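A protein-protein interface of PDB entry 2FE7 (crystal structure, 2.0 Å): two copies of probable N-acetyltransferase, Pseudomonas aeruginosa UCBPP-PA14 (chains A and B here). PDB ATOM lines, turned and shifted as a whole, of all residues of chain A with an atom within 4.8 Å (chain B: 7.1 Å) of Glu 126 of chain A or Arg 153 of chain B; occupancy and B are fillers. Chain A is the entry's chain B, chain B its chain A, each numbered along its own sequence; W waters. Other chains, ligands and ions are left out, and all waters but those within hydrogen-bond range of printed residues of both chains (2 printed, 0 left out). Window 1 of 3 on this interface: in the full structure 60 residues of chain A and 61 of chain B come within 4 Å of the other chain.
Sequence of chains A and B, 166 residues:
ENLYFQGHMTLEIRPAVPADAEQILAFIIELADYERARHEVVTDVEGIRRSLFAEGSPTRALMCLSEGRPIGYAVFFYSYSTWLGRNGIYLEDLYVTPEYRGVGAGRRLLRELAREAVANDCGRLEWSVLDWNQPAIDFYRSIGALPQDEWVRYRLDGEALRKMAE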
ATOM      1  N   SER A  79      27.495  -4.930 -12.553  1.00  0.00           N
ATOM      2  CA  SER A  79      27.067  -3.565 -12.296  1.00  0.00           C
ATOM      3  C   SER A  79      27.720  -3.100 -10.996  1.00  0.00           C
ATOM      4  O   SER A  79      28.496  -3.846 -10.383  1.00  0.00           O
ATOM      5  CB  SER A  79      25.535  -3.511 -12.179  1.00  0.00           C
ATOM      6  OG  SER A  79      25.107  -4.393 -11.158  1.00  0.00           O
ATOM      7  N   ILE A  89      25.161  -7.928 -10.365  1.00  0.00           N
ATOM      8  CA  ILE A  89      25.101  -8.534 -11.700  1.00  0.00           C
ATOM      9  C   ILE A  89      23.855  -8.042 -12.432  1.00  0.00           C
ATOM     10  O   ILE A  89      22.760  -7.984 -11.856  1.00  0.00           O
ATOM     11  CB  ILE A  89      25.128 -10.096 -11.649  1.00  0.00           C
ATOM     12  CG1 ILE A  89      26.497 -10.583 -11.151  1.00  0.00           C
ATOM     13  CG2 ILE A  89      24.849 -10.698 -13.035  1.00  0.00           C
ATOM     14  CD1 ILE A  89      26.570 -12.085 -10.896  1.00  0.00           C
ATOM     15  N   TYR A  90      24.033  -7.633 -13.686  1.00  0.00           N
ATOM     16  CA  TYR A  90      22.887  -7.294 -14.535  1.00  0.00           C
ATOM     17  C   TYR A  90      22.740  -8.333 -15.637  1.00  0.00           C
ATOM     18  O   TYR A  90      23.658  -8.533 -16.443  1.00  0.00           O
ATOM     19  CB  TYR A  90      23.013  -5.905 -15.160  1.00  0.00           C
ATOM     20  CG  TYR A  90      21.786  -5.515 -15.963  1.00  0.00           C
ATOM     21  CD1 TYR A  90      20.693  -4.908 -15.341  1.00  0.00           C
ATOM     22  CD2 TYR A  90      21.704  -5.766 -17.338  1.00  0.00           C
ATOM     23  CE1 TYR A  90      19.561  -4.542 -16.072  1.00  0.00           C
ATOM     24  CE2 TYR A  90      20.565  -5.403 -18.088  1.00  0.00           C
ATOM     25  CZ  TYR A  90      19.505  -4.790 -17.435  1.00  0.00           C
ATOM     26  OH  TYR A  90      18.383  -4.414 -18.133  1.00  0.00           O
ATOM     27  N   LEU A  91      21.586  -8.986 -15.652  1.00  0.00           N
ATOM     28  CA  LEU A  91      21.255  -9.962 -16.678  1.00  0.00           C
ATOM     29  C   LEU A  91      20.599  -9.290 -17.901  1.00  0.00           C
ATOM     30  O   LEU A  91      19.477  -8.777 -17.816  1.00  0.00           O
ATOM     31  CB  LEU A  91      20.357 -11.039 -16.060  1.00  0.00           C
ATOM     32  CG  LEU A  91      19.700 -12.083 -16.956  1.00  0.00           C
ATOM     33  CD1 LEU A  91      20.760 -12.939 -17.645  1.00  0.00           C
ATOM     34  CD2 LEU A  91      18.774 -12.944 -16.119  1.00  0.00           C
ATOM     35  N   ARG A 124      23.074  -7.036  -5.567  1.00  0.00           N
ATOM     36  CA  ARG A 124      21.878  -7.071  -6.418  1.00  0.00           C
ATOM     37  C   ARG A 124      22.055  -7.930  -7.664  1.00  0.00           C
ATOM     38  O   ARG A 124      23.132  -7.939  -8.287  1.00  0.00           O
ATOM     39  CB  ARG A 124      21.470  -5.634  -6.820  1.00  0.00           C
ATOM     40  CG  ARG A 124      21.642  -4.699  -5.634  1.00  0.00           C
ATOM     41  CD  ARG A 124      20.767  -3.520  -5.583  1.00  0.00           C
ATOM     42  NE  ARG A 124      21.286  -2.474  -6.406  1.00  0.00           N
ATOM     43  CZ  ARG A 124      21.279  -1.175  -6.123  1.00  0.00           C
ATOM     44  NH1 ARG A 124      20.820  -0.701  -4.971  1.00  0.00           N
ATOM     45  NH2 ARG A 124      21.771  -0.349  -7.029  1.00  0.00           N
ATOM     46  N   LEU A 125      21.006  -8.678  -7.988  1.00  0.00           N
ATOM     47  CA  LEU A 125      20.836  -9.239  -9.317  1.00  0.00           C
ATOM     48  C   LEU A 125      19.651  -8.515  -9.980  1.00  0.00           C
ATOM     49  O   LEU A 125      18.565  -8.414  -9.393  1.00  0.00           O
ATOM     50  CB  LEU A 125      20.617 -10.758  -9.251  1.00  0.00           C
ATOM     51  CG  LEU A 125      20.301 -11.489 -10.567  1.00  0.00           C
ATOM     52  CD1 LEU A 125      21.456 -11.437 -11.588  1.00  0.00           C
ATOM     53  CD2 LEU A 125      19.854 -12.936 -10.314  1.00  0.00           C
ATOM     54  N   GLU A 126      19.867  -8.004 -11.193  1.00  0.00           N
ATOM     55  CA  GLU A 126      18.860  -7.181 -11.877  1.00  0.00           C
ATOM     56  C   GLU A 126      18.749  -7.524 -13.358  1.00  0.00           C
ATOM     57  O   GLU A 126      19.647  -8.132 -13.935  1.00  0.00           O
ATOM     58  CB  GLU A 126      19.191  -5.682 -11.727  1.00  0.00           C
ATOM     59  CG  GLU A 126      19.113  -5.145 -10.288  1.00  0.00           C
ATOM     60  CD  GLU A 126      19.583  -3.717 -10.179  1.00  0.00           C
ATOM     61  OE1 GLU A 126      20.716  -3.421 -10.617  1.00  0.00           O
ATOM     62  OE2 GLU A 126      18.821  -2.884  -9.660  1.00  0.00           O
ATOM     63  N   TRP A 127      17.639  -7.123 -13.967  1.00  0.00           N
ATOM     64  CA  TRP A 127      17.378  -7.368 -15.375  1.00  0.00           C
ATOM     65  C   TRP A 127      16.213  -6.457 -15.733  1.00  0.00           C
ATOM     66  O   TRP A 127      15.678  -5.766 -14.869  1.00  0.00           O
ATOM     67  CB  TRP A 127      17.037  -8.848 -15.642  1.00  0.00           C
ATOM     68  CG  TRP A 127      15.861  -9.359 -14.861  1.00  0.00           C
ATOM     69  CD1 TRP A 127      14.554  -9.339 -15.250  1.00  0.00           C
ATOM     70  CD2 TRP A 127      15.884  -9.947 -13.559  1.00  0.00           C
ATOM     71  NE1 TRP A 127      13.755  -9.874 -14.262  1.00  0.00           N
ATOM     72  CE2 TRP A 127      14.550 -10.259 -13.216  1.00  0.00           C
ATOM     73  CE3 TRP A 127      16.910 -10.250 -12.642  1.00  0.00           C
ATOM     74  CZ2 TRP A 127      14.204 -10.861 -11.997  1.00  0.00           C
ATOM     75  CZ3 TRP A 127      16.569 -10.838 -11.433  1.00  0.00           C
ATOM     76  CH2 TRP A 127      15.220 -11.143 -11.120  1.00  0.00           C
ATOM     77  N   SER A 128      15.825  -6.454 -16.995  1.00  0.00           N
ATOM     78  CA  SER A 128      14.697  -5.632 -17.421  1.00  0.00           C
ATOM     79  C   SER A 128      13.669  -6.474 -18.142  1.00  0.00           C
ATOM     80  O   SER A 128      13.990  -7.525 -18.706  1.00  0.00           O
ATOM     81  CB  SER A 128      15.180  -4.483 -18.301  1.00  0.00           C
ATOM     82  OG  SER A 128      15.988  -3.603 -17.522  1.00  0.00           O
ATOM     83  N   LEU A 146      11.490  -7.387  -7.431  1.00  0.00           N
ATOM     84  CA  LEU A 146      10.652  -6.197  -7.260  1.00  0.00           C
ATOM     85  C   LEU A 146      10.948  -5.161  -8.342  1.00  0.00           C
ATOM     86  O   LEU A 146      12.112  -4.933  -8.670  1.00  0.00           O
ATOM     87  CB  LEU A 146      10.886  -5.577  -5.876  1.00  0.00           C
ATOM     88  CG  LEU A 146      10.635  -6.480  -4.669  1.00  0.00           C
ATOM     89  CD1 LEU A 146      11.050  -5.756  -3.383  1.00  0.00           C
ATOM     90  CD2 LEU A 146       9.170  -6.904  -4.610  1.00  0.00           C
ATOM     91  N   PRO A 147       9.899  -4.535  -8.883  1.00  0.00           N
ATOM     92  CA  PRO A 147      10.071  -3.562  -9.958  1.00  0.00           C
ATOM     93  C   PRO A 147      10.642  -2.248  -9.418  1.00  0.00           C
ATOM     94  O   PRO A 147      10.225  -1.776  -8.349  1.00  0.00           O
ATOM     95  CB  PRO A 147       8.643  -3.337 -10.468  1.00  0.00           C
ATOM     96  CG  PRO A 147       7.756  -3.639  -9.263  1.00  0.00           C
ATOM     97  CD  PRO A 147       8.482  -4.720  -8.498  1.00  0.00           C
ATOM     98  N   GLN A 148      11.586  -1.675 -10.157  1.00  0.00           N
ATOM     99  CA  GLN A 148      12.178  -0.379  -9.803  1.00  0.00           C
ATOM    100  C   GLN A 148      11.517   0.675 -10.679  1.00  0.00           C
ATOM    101  O   GLN A 148      12.156   1.291 -11.523  1.00  0.00           O
ATOM    102  CB  GLN A 148      13.703  -0.402  -9.985  1.00  0.00           C
ATOM    103  CG  GLN A 148      14.390  -1.604  -9.310  1.00  0.00           C
ATOM    104  CD  GLN A 148      14.128  -1.675  -7.815  1.00  0.00           C
ATOM    105  OE1 GLN A 148      13.540  -2.643  -7.303  1.00  0.00           O
ATOM    106  NE2 GLN A 148      14.558  -0.653  -7.103  1.00  0.00           N
ATOM    107  N   TRP A 151      12.287   4.669 -11.700  1.00  0.00           N
ATOM    108  CA  TRP A 151      13.403   5.029 -12.569  1.00  0.00           C
ATOM    109  C   TRP A 151      13.022   4.876 -14.031  1.00  0.00           C
ATOM    110  O   TRP A 151      12.305   3.934 -14.390  1.00  0.00           O
ATOM    111  CB  TRP A 151      14.625   4.165 -12.269  1.00  0.00           C
ATOM    112  CG  TRP A 151      15.192   4.390 -10.893  1.00  0.00           C
ATOM    113  CD1 TRP A 151      14.827   3.749  -9.741  1.00  0.00           C
ATOM    114  CD2 TRP A 151      16.207   5.334 -10.522  1.00  0.00           C
ATOM    115  NE1 TRP A 151      15.551   4.239  -8.672  1.00  0.00           N
ATOM    116  CE2 TRP A 151      16.414   5.203  -9.128  1.00  0.00           C
ATOM    117  CE3 TRP A 151      16.963   6.278 -11.232  1.00  0.00           C
ATOM    118  CZ2 TRP A 151      17.350   5.985  -8.428  1.00  0.00           C
ATOM    119  CZ3 TRP A 151      17.900   7.051 -10.538  1.00  0.00           C
ATOM    120  CH2 TRP A 151      18.076   6.902  -9.149  1.00  0.00           C
ATOM    121  N   ARG A 153      15.056   4.590 -17.758  1.00  0.00           N
ATOM    122  CA  ARG A 153      16.358   4.499 -18.412  1.00  0.00           C
ATOM    123  C   ARG A 153      16.431   5.443 -19.607  1.00  0.00           C
ATOM    124  O   ARG A 153      15.536   5.434 -20.440  1.00  0.00           O
ATOM    125  CB  ARG A 153      16.651   3.076 -18.882  1.00  0.00           C
ATOM    126  CG  ARG A 153      18.137   2.836 -19.093  1.00  0.00           C
ATOM    127  CD  ARG A 153      18.428   1.723 -20.065  1.00  0.00           C
ATOM    128  NE  ARG A 153      17.534   0.576 -19.945  1.00  0.00           N
ATOM    129  CZ  ARG A 153      17.484  -0.414 -20.837  1.00  0.00           C
ATOM    130  NH1 ARG A 153      18.288  -0.397 -21.902  1.00  0.00           N
ATOM    131  NH2 ARG A 153      16.631  -1.424 -20.674  1.00  0.00           N
ATOM    132  N   PHE B  77      30.188   1.775 -15.559  1.00  0.00           N
ATOM    133  CA  PHE B  77      30.681   0.442 -15.889  1.00  0.00           C
ATOM    134  C   PHE B  77      30.250   0.072 -17.301  1.00  0.00           C
ATOM    135  O   PHE B  77      29.386   0.731 -17.892  1.00  0.00           O
ATOM    136  CB  PHE B  77      30.206  -0.604 -14.854  1.00  0.00           C
ATOM    137  CG  PHE B  77      28.712  -0.588 -14.601  1.00  0.00           C
ATOM    138  CD1 PHE B  77      27.846  -1.318 -15.411  1.00  0.00           C
ATOM    139  CD2 PHE B  77      28.177   0.147 -13.544  1.00  0.00           C
ATOM    140  CE1 PHE B  77      26.471  -1.304 -15.189  1.00  0.00           C
ATOM    141  CE2 PHE B  77      26.790   0.160 -13.298  1.00  0.00           C
ATOM    142  CZ  PHE B  77      25.937  -0.570 -14.128  1.00  0.00           C
ATOM    143  N   TYR B  90      27.248   2.136 -18.997  1.00  0.00           N
ATOM    144  CA  TYR B  90      26.141   2.553 -18.150  1.00  0.00           C
ATOM    145  C   TYR B  90      26.680   3.488 -17.069  1.00  0.00           C
ATOM    146  O   TYR B  90      27.620   3.141 -16.350  1.00  0.00           O
ATOM    147  CB  TYR B  90      25.391   1.360 -17.550  1.00  0.00           C
ATOM    148  CG  TYR B  90      24.187   1.791 -16.747  1.00  0.00           C
ATOM    149  CD1 TYR B  90      22.961   2.004 -17.372  1.00  0.00           C
ATOM    150  CD2 TYR B  90      24.281   2.028 -15.370  1.00  0.00           C
ATOM    151  CE1 TYR B  90      21.852   2.418 -16.640  1.00  0.00           C
ATOM    152  CE2 TYR B  90      23.182   2.434 -14.633  1.00  0.00           C
ATOM    153  CZ  TYR B  90      21.974   2.625 -15.275  1.00  0.00           C
ATOM    154  OH  TYR B  90      20.870   3.034 -14.571  1.00  0.00           O
ATOM    155  N   GLU B  92      26.137   5.133 -13.674  1.00  0.00           N
ATOM    156  CA  GLU B  92      25.370   4.899 -12.439  1.00  0.00           C
ATOM    157  C   GLU B  92      25.092   6.194 -11.661  1.00  0.00           C
ATOM    158  O   GLU B  92      23.954   6.456 -11.263  1.00  0.00           O
ATOM    159  CB  GLU B  92      26.065   3.858 -11.542  1.00  0.00           C
ATOM    160  CG  GLU B  92      25.422   3.656 -10.153  1.00  0.00           C
ATOM    161  CD  GLU B  92      23.906   3.396 -10.212  1.00  0.00           C
ATOM    162  OE1 GLU B  92      23.444   2.618 -11.073  1.00  0.00           O
ATOM    163  OE2 GLU B  92      23.169   3.991  -9.405  1.00  0.00           O
ATOM    164  N   TRP B 127      21.857   5.595 -18.696  1.00  0.00           N
ATOM    165  CA  TRP B 127      21.788   5.984 -17.292  1.00  0.00           C
ATOM    166  C   TRP B 127      20.309   6.017 -16.928  1.00  0.00           C
ATOM    167  O   TRP B 127      19.435   5.845 -17.803  1.00  0.00           O
ATOM    168  CB  TRP B 127      22.446   7.357 -17.047  1.00  0.00           C
ATOM    169  CG  TRP B 127      21.790   8.486 -17.779  1.00  0.00           C
ATOM    170  CD1 TRP B 127      20.732   9.247 -17.347  1.00  0.00           C
ATOM    171  CD2 TRP B 127      22.141   8.985 -19.074  1.00  0.00           C
ATOM    172  NE1 TRP B 127      20.397  10.179 -18.310  1.00  0.00           N
ATOM    173  CE2 TRP B 127      21.245  10.039 -19.377  1.00  0.00           C
ATOM    174  CE3 TRP B 127      23.120   8.642 -20.016  1.00  0.00           C
ATOM    175  CZ2 TRP B 127      21.320  10.770 -20.572  1.00  0.00           C
ATOM    176  CZ3 TRP B 127      23.180   9.355 -21.217  1.00  0.00           C
ATOM    177  CH2 TRP B 127      22.284  10.406 -21.480  1.00  0.00           C
ATOM    178  N   SER B 128      20.024   6.234 -15.652  1.00  0.00           N
ATOM    179  CA  SER B 128      18.643   6.248 -15.218  1.00  0.00           C
ATOM    180  C   SER B 128      18.323   7.522 -14.480  1.00  0.00           C
ATOM    181  O   SER B 128      19.221   8.185 -13.951  1.00  0.00           O
ATOM    182  CB  SER B 128      18.334   5.003 -14.388  1.00  0.00           C
ATOM    183  OG  SER B 128      18.428   3.841 -15.214  1.00  0.00           O
ATOM    184  N   VAL B 129      17.044   7.875 -14.464  1.00  0.00           N
ATOM    185  CA  VAL B 129      16.588   9.072 -13.781  1.00  0.00           C
ATOM    186  C   VAL B 129      15.256   8.783 -13.095  1.00  0.00           C
ATOM    187  O   VAL B 129      14.416   8.019 -13.609  1.00  0.00           O
ATOM    188  CB  VAL B 129      16.487  10.295 -14.747  1.00  0.00           C
ATOM    189  CG1 VAL B 129      15.421  10.089 -15.795  1.00  0.00           C
ATOM    190  CG2 VAL B 129      16.234  11.594 -13.984  1.00  0.00           C
ATOM    191  N   TRP B 151      10.568  -0.571 -20.876  1.00  0.00           N
ATOM    192  CA  TRP B 151      11.206  -1.547 -19.991  1.00  0.00           C
ATOM    193  C   TRP B 151      10.991  -1.198 -18.532  1.00  0.00           C
ATOM    194  O   TRP B 151      10.962  -0.021 -18.169  1.00  0.00           O
ATOM    195  CB  TRP B 151      12.711  -1.611 -20.269  1.00  0.00           C
ATOM    196  CG  TRP B 151      13.065  -2.103 -21.655  1.00  0.00           C
ATOM    197  CD1 TRP B 151      13.265  -1.337 -22.775  1.00  0.00           C
ATOM    198  CD2 TRP B 151      13.256  -3.466 -22.061  1.00  0.00           C
ATOM    199  NE1 TRP B 151      13.568  -2.144 -23.855  1.00  0.00           N
ATOM    200  CE2 TRP B 151      13.577  -3.452 -23.445  1.00  0.00           C
ATOM    201  CE3 TRP B 151      13.199  -4.698 -21.393  1.00  0.00           C
ATOM    202  CZ2 TRP B 151      13.827  -4.623 -24.172  1.00  0.00           C
ATOM    203  CZ3 TRP B 151      13.451  -5.872 -22.122  1.00  0.00           C
ATOM    204  CH2 TRP B 151      13.757  -5.820 -23.496  1.00  0.00           C
ATOM    205  N   VAL B 152      10.859  -2.225 -17.698  1.00  0.00           N
ATOM    206  CA  VAL B 152      10.859  -2.061 -16.245  1.00  0.00           C
ATOM    207  C   VAL B 152      12.049  -2.838 -15.679  1.00  0.00           C
ATOM    208  O   VAL B 152      12.196  -4.016 -15.973  1.00  0.00           O
ATOM    209  CB  VAL B 152       9.543  -2.605 -15.628  1.00  0.00           C
ATOM    210  CG1 VAL B 152       9.559  -2.469 -14.116  1.00  0.00           C
ATOM    211  CG2 VAL B 152       8.336  -1.865 -16.203  1.00  0.00           C
ATOM    212  N   ARG B 153      12.890  -2.188 -14.874  1.00  0.00           N
ATOM    213  CA  ARG B 153      14.016  -2.870 -14.232  1.00  0.00           C
ATOM    214  C   ARG B 153      13.508  -3.687 -13.049  1.00  0.00           C
ATOM    215  O   ARG B 153      12.789  -3.160 -12.208  1.00  0.00           O
ATOM    216  CB  ARG B 153      15.059  -1.852 -13.751  1.00  0.00           C
ATOM    217  CG  ARG B 153      16.278  -2.434 -13.004  1.00  0.00           C
ATOM    218  CD  ARG B 153      17.364  -1.363 -12.710  1.00  0.00           C
ATOM    219  NE  ARG B 153      17.285  -0.279 -13.686  1.00  0.00           N
ATOM    220  CZ  ARG B 153      16.742   0.921 -13.452  1.00  0.00           C
ATOM    221  NH1 ARG B 153      16.267   1.212 -12.239  1.00  0.00           N
ATOM    222  NH2 ARG B 153      16.689   1.840 -14.436  1.00  0.00           N
ATOM    223  N   TYR B 154      13.869  -4.967 -13.000  1.00  0.00           N
ATOM    224  CA  TYR B 154      13.549  -5.811 -11.832  1.00  0.00           C
ATOM    225  C   TYR B 154      14.800  -6.115 -11.036  1.00  0.00           C
ATOM    226  O   TYR B 154      15.896  -6.141 -11.575  1.00  0.00           O
ATOM    227  CB  TYR B 154      12.835  -7.105 -12.238  1.00  0.00           C
ATOM    228  CG  TYR B 154      11.336  -6.954 -12.218  1.00  0.00           C
ATOM    229  CD1 TYR B 154      10.672  -6.254 -13.233  1.00  0.00           C
ATOM    230  CD2 TYR B 154      10.578  -7.481 -11.167  1.00  0.00           C
ATOM    231  CE1 TYR B 154       9.285  -6.098 -13.209  1.00  0.00           C
ATOM    232  CE2 TYR B 154       9.194  -7.332 -11.129  1.00  0.00           C
ATOM    233  CZ  TYR B 154       8.559  -6.645 -12.150  1.00  0.00           C
ATOM    234  OH  TYR B 154       7.204  -6.490 -12.116  1.00  0.00           O
ATOM    235  N   ARG B 155      14.625  -6.360  -9.749  1.00  0.00           N
ATOM    236  CA  ARG B 155      15.753  -6.522  -8.843  1.00  0.00           C
ATOM    237  C   ARG B 155      15.474  -7.583  -7.794  1.00  0.00           C
ATOM    238  O   ARG B 155      14.404  -7.618  -7.203  1.00  0.00           O
ATOM    239  CB  ARG B 155      16.058  -5.188  -8.150  1.00  0.00           C
ATOM    240  CG  ARG B 155      17.073  -5.263  -7.017  1.00  0.00           C
ATOM    241  CD  ARG B 155      17.178  -3.936  -6.257  1.00  0.00           C
ATOM    242  NE  ARG B 155      17.708  -2.875  -7.109  1.00  0.00           N
ATOM    243  CZ  ARG B 155      17.875  -1.606  -6.732  1.00  0.00           C
ATOM    244  NH1 ARG B 155      18.363  -0.728  -7.602  1.00  0.00           N
ATOM    245  NH2 ARG B 155      17.549  -1.211  -5.503  1.00  0.00           N
ATOM    246  N   LEU B 156      16.446  -8.454  -7.567  1.00  0.00           N
ATOM    247  CA  LEU B 156      16.457  -9.214  -6.328  1.00  0.00           C
ATOM    248  C   LEU B 156      17.676  -8.838  -5.508  1.00  0.00           C
ATOM    249  O   LEU B 156      18.792  -8.679  -6.033  1.00  0.00           O
ATOM    250  CB  LEU B 156      16.321 -10.735  -6.527  1.00  0.00           C
ATOM    251  CG  LEU B 156      16.662 -11.462  -7.804  1.00  0.00           C
ATOM    252  CD1 LEU B 156      18.130 -11.267  -7.960  1.00  0.00           C
ATOM    253  CD2 LEU B 156      16.337 -12.953  -7.724  1.00  0.00           C
ATOM    254  N   LEU B 161      17.206 -12.551  -2.754  1.00  0.00           N
ATOM    255  CA  LEU B 161      18.393 -12.951  -3.509  1.00  0.00           C
ATOM    256  C   LEU B 161      19.049 -14.191  -2.892  1.00  0.00           C
ATOM    257  O   LEU B 161      19.345 -15.149  -3.597  1.00  0.00           O
ATOM    258  CB  LEU B 161      19.409 -11.807  -3.607  1.00  0.00           C
ATOM    259  CG  LEU B 161      20.728 -12.122  -4.348  1.00  0.00           C
ATOM    260  CD1 LEU B 161      20.473 -12.494  -5.817  1.00  0.00           C
ATOM    261  CD2 LEU B 161      21.716 -10.961  -4.258  1.00  0.00           C
HETATM  262  O   HOH W   1      12.353   0.506 -14.248  1.00  0.00           O
HETATM  263  O   HOH W   2      12.954   2.780 -18.384  1.00  0.00           O
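The backbone carbonyl oxygen (O) of Arg 153 of chain B lies within hydrogen-bond range of the backbone NH (N) of Gln 148 of chain A (2.8 Å).
N of Tyr 154 of chain B is in hydrogen-bond range of O of Trp 127 of chain A (2.7 Å).
OE2 of Glu 126 of chain A is in salt-bridge range of NE of Arg 155 of chain B.
The backbone NH (N) of Leu 146 of chain A lies within hydrogen-bond range of the backbone carbonyl oxygen (O) of Arg 155 of chain B.
The side-chain amide nitrogen (NE2) of Gln 148 of chain A sits close to the guanidinium group (NH2) of Arg 155 of chain B (3.4 Å).
N of Leu 156 of chain B lies within hydrogen-bond range of O of Leu 125 of chain A (2.8 Å).
NH2 of Arg 155 of chain B lies close to NH1 of Arg 124 of chain A.
N of Tyr 90 of chain B is in hydrogen-bond range of O of Phe 77 of chain B, 2.8 Å away.
The side-chain hydroxyl (OG) of Ser 128 of chain B is in hydrogen-bond range of the guanidinium group (NH2) of Arg 153 of chain B (2.8 Å).
The backbone NH (N) of Ile 89 of chain A sits at hydrogen-bond distance from the backbone carbonyl oxygen (O) of Arg 124 of chain A, at 2.9 Å.
N of Glu 126 of chain A is in hydrogen-bond range of O of Ile 89 of chain A.
The side-chain hydroxyl (OH) of Tyr 90 of chain A sits at hydrogen-bond distance from the side-chain hydroxyl (OG) of Ser 128 of chain A, at 2.6 Å.
The backbone NH (N) of Leu 91 of chain A is in hydrogen-bond range of the backbone carbonyl oxygen (O) of Glu 126 of chain A.
Among the printed residues, pairs that only touch across the chains: Glu 126 of chain A with Tyr 154 of chain B, Ser 128 of chain A with Val 152 of chain B, Trp 151 of chain A with Val 129 of chain B, Trp 151 of chain A with Arg 153 of chain B, Trp 127 of chain A with Arg 153 of chain B, Arg 153 of chain A with Trp 127 of chain B, Leu 125 of chain A with Arg 155 of chain B, Arg 124 of chain A with Leu 156 of chain B, Ser 79 of chain A with Phe 77 of chain B, Pro 147 of chain A with Arg 153 of chain B, Leu 146 of chain A with Tyr 154 of chain B, Trp 127 of chain A with Leu 156 of chain B, Pro 147 of chain A with Tyr 154 of chain B, Trp 151 of chain A with Ser 128 of chain B, Ser 128 of chain A with Trp 151 of chain B, Glu 126 of chain A with Arg 153 of chain B, Arg 153 of chain A with Trp 151 of chain B, Leu 125 of chain A with Leu 161 of chain B, Pro 147 of chain A with Val 152 of chain B, Arg 153 of chain A with Ser 128 of chain B and Ser 128 of chain A with Arg 153 of chain B.
Printed residues of chain B within 4 Å of Ser 79 of chain A: Phe 77.
Tyr 90 of chain A touches none of the printed residues of chain B.
Printed residues of chain B within 4 Å of Ser 128 of chain A: Trp 151 (3.7 Å), Val 152 (3.3 Å) and Arg 153 (3.9 Å).
Printed residues of chain B within 4 Å of Leu 146 of chain A: Tyr 154 (3.6 Å) and Arg 155 (2.9 Å).
Printed residues of chain A within 4 Å of Ser 128 of chain B: Trp 151 (3.7 Å) and Arg 153 (3.9 Å).
Printed residues of chain A within 4 Å of Arg 153 of chain B: Glu 126 (3.7 Å), Trp 127 (3.4 Å), Ser 128 (3.9 Å), Pro 147 (3.6 Å), Gln 148 (2.8 Å) and Trp 151 (3.4 Å).
Of the printed residues of chain A, Tyr 154 of chain B touches Glu 126 (3.2 Å), Trp 127 (2.7 Å), Leu 146 (3.6 Å) and Pro 147 (3.7 Å).
The nearest residue of chain B that does not touch Glu 126 of chain A is Leu 156 of chain B (4.9 Å).
The nearest printed residue of chain A that does not touch Arg 153 of chain B is Leu 146 of chain A (4.01 Å).
The nearest printed residue of chain B that does not touch Trp 151 of chain A is Trp 151 of chain B (5.6 Å).
Hydrophobic or aromatic side chains of chain B that line the printed part of chain A: Phe 77, Trp 151, Val 152, Tyr 154, Leu 156 and Leu 161.
Of the 14 printed residues of chain A, 11 touch a printed residue of chain B.
Printed residues of chain A that touch a printed residue of chain B: Ser 79, Arg 124, Leu 125, Glu 126, Trp 127, Ser 128, Leu 146, Pro 147, Gln 148, Trp 151 and Arg 153.
Hydrophobic or aromatic side chains of chain A that line the printed part of chain B: Leu 125, Trp 127, Pro 147 and Trp 151.
Along chain A the printed residues that touch a printed residue of chain B span positions 79 to 153.
Among the printed residues, Asp or Glu carboxylates within 4 Å of a Lys or Arg side-chain nitrogen of the other chain: Glu 126 of chain A with Arg 155 of chain B.
Trp 127 of chain A touches Arg 153 of chain B, and with the chains exchanged Arg 153 of chain A touches Trp 127 of chain B.
Ser 128 of chain A touches Trp 151 of chain B, and with the chains exchanged Trp 151 of chain A touches Ser 128 of chain B.
Ser 128 of chain A touches Arg 153 of chain B, and with the chains exchanged Arg 153 of chain A touches Ser 128 of chain B.
Trp 151 of chain A touches Arg 153 of chain B, and with the chains exchanged Arg 153 of chain A touches Trp 151 of chain B.
Positions printed for both chains: 90, 127, 128, 151 and 153.
Water W1 lies within hydrogen-bond range of N of Arg 153 of chain B (2.8 Å), O of Gln 148 of chain A (2.8 Å) and O of Trp 151 of chain A (3.4 Å).
Water W2 lies within hydrogen-bond range of N of Arg 153 of chain A (2.8 Å) and O of Trp 151 of chain B (3.4 Å).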
